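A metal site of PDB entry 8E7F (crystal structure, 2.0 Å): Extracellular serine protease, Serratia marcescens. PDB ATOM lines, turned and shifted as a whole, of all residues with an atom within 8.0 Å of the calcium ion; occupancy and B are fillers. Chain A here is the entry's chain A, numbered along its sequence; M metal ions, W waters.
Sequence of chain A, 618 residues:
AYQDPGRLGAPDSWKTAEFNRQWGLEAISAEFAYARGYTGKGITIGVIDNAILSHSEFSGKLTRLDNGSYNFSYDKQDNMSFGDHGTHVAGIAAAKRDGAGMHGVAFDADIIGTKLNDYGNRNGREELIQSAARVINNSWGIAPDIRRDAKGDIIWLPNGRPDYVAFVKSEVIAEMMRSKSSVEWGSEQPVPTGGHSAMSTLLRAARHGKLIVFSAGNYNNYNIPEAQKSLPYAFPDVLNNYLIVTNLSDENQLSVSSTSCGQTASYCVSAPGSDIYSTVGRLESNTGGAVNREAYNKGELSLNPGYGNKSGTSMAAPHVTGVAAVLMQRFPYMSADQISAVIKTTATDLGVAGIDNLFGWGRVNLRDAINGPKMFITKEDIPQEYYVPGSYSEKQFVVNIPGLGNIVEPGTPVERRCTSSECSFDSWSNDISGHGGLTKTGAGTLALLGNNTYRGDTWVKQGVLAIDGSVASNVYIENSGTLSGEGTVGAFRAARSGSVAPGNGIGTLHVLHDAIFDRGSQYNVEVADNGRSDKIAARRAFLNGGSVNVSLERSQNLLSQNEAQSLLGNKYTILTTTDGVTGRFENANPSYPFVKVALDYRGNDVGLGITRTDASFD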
ATOM      1  N   SER A 484       2.633  22.521 -29.512  1.00  0.00           N
ATOM      2  CA  SER A 484       3.147  21.428 -28.647  1.00  0.00           C
ATOM      3  C   SER A 484       3.021  20.092 -29.399  1.00  0.00           C
ATOM      4  O   SER A 484       2.553  20.093 -30.566  1.00  0.00           O
ATOM      5  CB  SER A 484       2.422  21.419 -27.323  1.00  0.00           C
ATOM      6  OG  SER A 484       3.235  20.915 -26.275  1.00  0.00           O
ATOM      7  N   GLY A 485       3.438  18.989 -28.770  1.00  0.00           N
ATOM      8  CA  GLY A 485       3.223  17.627 -29.292  1.00  0.00           C
ATOM      9  C   GLY A 485       4.478  16.936 -29.787  1.00  0.00           C
ATOM     10  O   GLY A 485       5.510  17.569 -29.970  1.00  0.00           O
ATOM     11  N   VAL A 500       6.754  27.681 -28.672  1.00  0.00           N
ATOM     12  CA  VAL A 500       6.832  26.248 -29.063  1.00  0.00           C
ATOM     13  C   VAL A 500       7.283  25.444 -27.829  1.00  0.00           C
ATOM     14  O   VAL A 500       8.247  25.830 -27.183  1.00  0.00           O
ATOM     15  CB  VAL A 500       7.760  26.061 -30.265  1.00  0.00           C
ATOM     16  CG1 VAL A 500       7.819  24.602 -30.687  1.00  0.00           C
ATOM     17  CG2 VAL A 500       7.366  26.950 -31.417  1.00  0.00           C
ATOM     18  N   ALA A 501       6.549  24.386 -27.508  1.00  0.00           N
ATOM     19  CA  ALA A 501       6.789  23.498 -26.347  1.00  0.00           C
ATOM     20  C   ALA A 501       6.721  22.058 -26.816  1.00  0.00           C
ATOM     21  O   ALA A 501       5.694  21.402 -26.663  1.00  0.00           O
ATOM     22  CB  ALA A 501       5.780  23.775 -25.266  1.00  0.00           C
ATOM     23  N   PRO A 502       7.817  21.485 -27.390  1.00  0.00           N
ATOM     24  CA  PRO A 502       7.774  20.164 -28.012  1.00  0.00           C
ATOM     25  C   PRO A 502       7.383  19.107 -26.988  1.00  0.00           C
ATOM     26  O   PRO A 502       7.571  19.345 -25.832  1.00  0.00           O
ATOM     27  CB  PRO A 502       9.200  19.902 -28.473  1.00  0.00           C
ATOM     28  CG  PRO A 502       9.819  21.279 -28.553  1.00  0.00           C
ATOM     29  CD  PRO A 502       9.173  22.055 -27.421  1.00  0.00           C
ATOM     30  N   GLY A 503       6.835  17.986 -27.470  1.00  0.00           N
ATOM     31  CA  GLY A 503       6.466  16.802 -26.675  1.00  0.00           C
ATOM     32  C   GLY A 503       5.221  17.042 -25.851  1.00  0.00           C
ATOM     33  O   GLY A 503       4.653  18.166 -25.907  1.00  0.00           O
ATOM     34  N   ASN A 504       4.802  15.995 -25.133  1.00  0.00           N
ATOM     35  CA  ASN A 504       3.834  16.004 -24.009  1.00  0.00           C
ATOM     36  C   ASN A 504       4.668  15.699 -22.774  1.00  0.00           C
ATOM     37  O   ASN A 504       4.861  14.500 -22.435  1.00  0.00           O
ATOM     38  CB  ASN A 504       2.685  15.007 -24.249  1.00  0.00           C
ATOM     39  CG  ASN A 504       2.126  15.092 -25.660  1.00  0.00           C
ATOM     40  OD1 ASN A 504       1.641  16.146 -26.074  1.00  0.00           O
ATOM     41  ND2 ASN A 504       2.198  14.001 -26.402  1.00  0.00           N
ATOM     42  N   GLY A 505       5.242  16.745 -22.188  1.00  0.00           N
ATOM     43  CA  GLY A 505       6.492  16.654 -21.408  1.00  0.00           C
ATOM     44  C   GLY A 505       7.687  16.602 -22.352  1.00  0.00           C
ATOM     45  O   GLY A 505       7.650  17.310 -23.372  1.00  0.00           O
ATOM     46  N   ILE A 506       8.688  15.773 -22.054  1.00  0.00           N
ATOM     47  CA  ILE A 506       9.923  15.692 -22.875  1.00  0.00           C
ATOM     48  C   ILE A 506       9.588  14.923 -24.150  1.00  0.00           C
ATOM     49  O   ILE A 506       9.140  13.779 -24.058  1.00  0.00           O
ATOM     50  CB  ILE A 506      11.093  15.060 -22.105  1.00  0.00           C
ATOM     51  CG1 ILE A 506      11.587  16.021 -21.022  1.00  0.00           C
ATOM     52  CG2 ILE A 506      12.206  14.637 -23.050  1.00  0.00           C
ATOM     53  CD1 ILE A 506      12.617  15.444 -20.097  1.00  0.00           C
ATOM     54  N   GLY A 507       9.805  15.560 -25.284  1.00  0.00           N
ATOM     55  CA  GLY A 507       9.544  14.925 -26.580  1.00  0.00           C
ATOM     56  C   GLY A 507      10.144  15.719 -27.705  1.00  0.00           C
ATOM     57  O   GLY A 507      10.662  16.836 -27.470  1.00  0.00           O
ATOM     58  N   THR A 508      10.067  15.165 -28.897  1.00  0.00           N
ATOM     59  CA  THR A 508      10.582  15.815 -30.114  1.00  0.00           C
ATOM     60  C   THR A 508       9.411  16.246 -30.992  1.00  0.00           C
ATOM     61  O   THR A 508       8.530  15.424 -31.220  1.00  0.00           O
ATOM     62  CB  THR A 508      11.522  14.889 -30.883  1.00  0.00           C
ATOM     63  OG1 THR A 508      12.609  14.622 -30.000  1.00  0.00           O
ATOM     64  CG2 THR A 508      12.003  15.527 -32.172  1.00  0.00           C
ATOM     65  N   TYR A 523      10.774  29.514 -26.825  1.00  0.00           N
ATOM     66  CA  TYR A 523      11.011  28.061 -26.944  1.00  0.00           C
ATOM     67  C   TYR A 523      11.133  27.500 -25.521  1.00  0.00           C
ATOM     68  O   TYR A 523      12.170  27.758 -24.850  1.00  0.00           O
ATOM     69  CB  TYR A 523      12.215  27.835 -27.865  1.00  0.00           C
ATOM     70  CG  TYR A 523      12.593  26.384 -28.096  1.00  0.00           C
ATOM     71  CD1 TYR A 523      11.740  25.361 -27.730  1.00  0.00           C
ATOM     72  CD2 TYR A 523      13.799  26.040 -28.669  1.00  0.00           C
ATOM     73  CE1 TYR A 523      12.081  24.036 -27.921  1.00  0.00           C
ATOM     74  CE2 TYR A 523      14.165  24.725 -28.871  1.00  0.00           C
ATOM     75  CZ  TYR A 523      13.312  23.711 -28.475  1.00  0.00           C
ATOM     76  OH  TYR A 523      13.626  22.391 -28.647  1.00  0.00           O
ATOM     77  N   ASN A 524      10.088  26.800 -25.051  1.00  0.00           N
ATOM     78  CA  ASN A 524      10.031  26.200 -23.698  1.00  0.00           C
ATOM     79  C   ASN A 524      10.583  24.778 -23.726  1.00  0.00           C
ATOM     80  O   ASN A 524       9.846  23.803 -24.099  1.00  0.00           O
ATOM     81  CB  ASN A 524       8.624  26.294 -23.090  1.00  0.00           C
ATOM     82  CG  ASN A 524       8.124  27.723 -22.953  1.00  0.00           C
ATOM     83  OD1 ASN A 524       8.908  28.647 -22.887  1.00  0.00           O
ATOM     84  ND2 ASN A 524       6.816  27.912 -22.926  1.00  0.00           N
ATOM     85  N   VAL A 525      11.842  24.632 -23.304  1.00  0.00           N
ATOM     86  CA  VAL A 525      12.612  23.363 -23.307  1.00  0.00           C
ATOM     87  C   VAL A 525      12.522  22.736 -21.906  1.00  0.00           C
ATOM     88  O   VAL A 525      12.904  23.409 -20.907  1.00  0.00           O
ATOM     89  CB  VAL A 525      14.077  23.587 -23.733  1.00  0.00           C
ATOM     90  CG1 VAL A 525      14.890  22.295 -23.661  1.00  0.00           C
ATOM     91  CG2 VAL A 525      14.183  24.207 -25.106  1.00  0.00           C
ATOM     92  N   GLU A 526      12.011  21.509 -21.829  1.00  0.00           N
ATOM     93  CA  GLU A 526      12.125  20.627 -20.648  1.00  0.00           C
ATOM     94  C   GLU A 526      13.424  19.823 -20.768  1.00  0.00           C
ATOM     95  O   GLU A 526      13.748  19.369 -21.869  1.00  0.00           O
ATOM     96  CB  GLU A 526      10.865  19.773 -20.503  1.00  0.00           C
ATOM     97  CG  GLU A 526       9.636  20.595 -20.087  1.00  0.00           C
ATOM     98  CD  GLU A 526       8.283  19.913 -20.259  1.00  0.00           C
ATOM     99  OE1 GLU A 526       7.997  19.424 -21.373  1.00  0.00           O
ATOM    100  OE2 GLU A 526       7.515  19.903 -19.286  1.00  0.00           O
ATOM    101  N   VAL A 527      14.181  19.708 -19.676  1.00  0.00           N
ATOM    102  CA  VAL A 527      15.428  18.909 -19.564  1.00  0.00           C
ATOM    103  C   VAL A 527      15.271  17.911 -18.417  1.00  0.00           C
ATOM    104  O   VAL A 527      14.475  18.190 -17.473  1.00  0.00           O
ATOM    105  CB  VAL A 527      16.654  19.801 -19.328  1.00  0.00           C
ATOM    106  CG1 VAL A 527      16.932  20.719 -20.521  1.00  0.00           C
ATOM    107  CG2 VAL A 527      16.525  20.610 -18.055  1.00  0.00           C
ATOM    108  N   SER A 533      16.207  15.880 -23.313  1.00  0.00           N
ATOM    109  CA  SER A 533      15.491  17.175 -23.408  1.00  0.00           C
ATOM    110  C   SER A 533      14.484  17.183 -24.554  1.00  0.00           C
ATOM    111  O   SER A 533      14.498  16.270 -25.389  1.00  0.00           O
ATOM    112  CB  SER A 533      16.437  18.315 -23.560  1.00  0.00           C
ATOM    113  OG  SER A 533      17.077  18.273 -24.824  1.00  0.00           O
ATOM    114  N   ASP A 534      13.625  18.194 -24.552  1.00  0.00           N
ATOM    115  CA  ASP A 534      12.819  18.625 -25.715  1.00  0.00           C
ATOM    116  C   ASP A 534      13.764  18.898 -26.880  1.00  0.00           C
ATOM    117  O   ASP A 534      14.940  19.222 -26.669  1.00  0.00           O
ATOM    118  CB  ASP A 534      11.988  19.854 -25.392  1.00  0.00           C
ATOM    119  CG  ASP A 534      10.801  19.565 -24.497  1.00  0.00           C
ATOM    120  OD1 ASP A 534      10.352  18.388 -24.441  1.00  0.00           O
ATOM    121  OD2 ASP A 534      10.313  20.532 -23.868  1.00  0.00           O
ATOM    122  N   LYS A 535      13.245  18.749 -28.083  1.00  0.00           N
ATOM    123  CA  LYS A 535      14.017  18.971 -29.318  1.00  0.00           C
ATOM    124  C   LYS A 535      13.029  19.314 -30.434  1.00  0.00           C
ATOM    125  O   LYS A 535      11.920  18.773 -30.492  1.00  0.00           O
ATOM    126  CB  LYS A 535      14.835  17.719 -29.654  1.00  0.00           C
ATOM    127  CG  LYS A 535      15.696  17.864 -30.892  1.00  0.00           C
ATOM    128  CD  LYS A 535      16.597  16.677 -31.184  1.00  0.00           C
ATOM    129  CE  LYS A 535      15.845  15.374 -31.321  1.00  0.00           C
ATOM    130  NZ  LYS A 535      16.624  14.384 -32.087  1.00  0.00           N
ATOM    131  N   SER A 551      13.167  24.448 -18.050  1.00  0.00           N
ATOM    132  CA  SER A 551      12.546  23.930 -16.814  1.00  0.00           C
ATOM    133  C   SER A 551      12.694  22.414 -16.781  1.00  0.00           C
ATOM    134  O   SER A 551      12.997  21.829 -17.827  1.00  0.00           O
ATOM    135  CB  SER A 551      11.104  24.334 -16.712  1.00  0.00           C
ATOM    136  OG  SER A 551      10.328  23.723 -17.741  1.00  0.00           O
ATOM    137  N   LEU A 552      12.459  21.801 -15.624  1.00  0.00           N
ATOM    138  CA  LEU A 552      12.337  20.332 -15.499  1.00  0.00           C
ATOM    139  C   LEU A 552      10.999  19.935 -16.103  1.00  0.00           C
ATOM    140  O   LEU A 552      10.139  20.825 -16.300  1.00  0.00           O
ATOM    141  CB  LEU A 552      12.451  19.933 -14.032  1.00  0.00           C
ATOM    142  CG  LEU A 552      13.833  20.127 -13.389  1.00  0.00           C
ATOM    143  CD1 LEU A 552      13.819  19.701 -11.938  1.00  0.00           C
ATOM    144  CD2 LEU A 552      14.903  19.361 -14.140  1.00  0.00           C
ATOM    145  N   GLU A 553      10.840  18.635 -16.377  1.00  0.00           N
ATOM    146  CA  GLU A 553       9.675  18.061 -17.099  1.00  0.00           C
ATOM    147  C   GLU A 553       8.422  18.329 -16.268  1.00  0.00           C
ATOM    148  O   GLU A 553       8.419  17.953 -15.089  1.00  0.00           O
ATOM    149  CB  GLU A 553       9.865  16.571 -17.345  1.00  0.00           C
ATOM    150  CG  GLU A 553       8.735  15.945 -18.154  1.00  0.00           C
ATOM    151  CD  GLU A 553       9.003  14.538 -18.636  1.00  0.00           C
ATOM    152  OE1 GLU A 553      10.052  13.953 -18.255  1.00  0.00           O
ATOM    153  OE2 GLU A 553       8.162  14.020 -19.416  1.00  0.00           O
ATOM    154  N   ARG A 554       7.436  18.983 -16.879  1.00  0.00           N
ATOM    155  CA  ARG A 554       6.065  19.234 -16.359  1.00  0.00           C
ATOM    156  C   ARG A 554       6.146  20.142 -15.135  1.00  0.00           C
ATOM    157  O   ARG A 554       5.177  20.184 -14.385  1.00  0.00           O
ATOM    158  CB  ARG A 554       5.350  17.903 -16.072  1.00  0.00           C
ATOM    159  CG  ARG A 554       4.469  17.432 -17.225  1.00  0.00           C
ATOM    160  CD  ARG A 554       3.800  16.125 -16.884  1.00  0.00           C
ATOM    161  NE  ARG A 554       4.709  15.022 -17.110  1.00  0.00           N
ATOM    162  CZ  ARG A 554       4.823  14.339 -18.254  1.00  0.00           C
ATOM    163  NH1 ARG A 554       4.067  14.636 -19.298  1.00  0.00           N
ATOM    164  NH2 ARG A 554       5.703  13.348 -18.343  1.00  0.00           N
HETATM  165 CA    CA M   1       8.162  19.515 -23.613  1.00  0.00          CA
HETATM  166  O   HOH W   1       8.036  21.930 -23.455  1.00  0.00           O
HETATM  167  O   HOH W   2       5.786  19.727 -23.875  1.00  0.00           O
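N of Arg 554 sits at hydrogen-bond distance from OE2 of Glu 526 (2.6 Å). OD1 of Asp 534 lies close to N of Gly 507, at 3.0 Å.
Within 4 Å of the calcium ion: Pro 502, Gly 505, Glu 526 and Asp 534. The nearest printed residue that does not touch the calcium ion is Ile 506 (4.1 Å).
OE1 of Glu 526 binds the calcium ion (2.2 Å). The calcium ion is bound by O of Gly 505. The backbone carbonyl oxygen (O) of Pro 502 binds the calcium ion. The side-chain carboxylate (OD2) of Asp 534 binds the calcium ion (2.4 Å). Water W2 is bound to the calcium ion (2.4 Å). The calcium ion is bound by water W1 (2.4 Å). OD1 of Asp 534 is bound to the calcium ion (2.6 Å).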
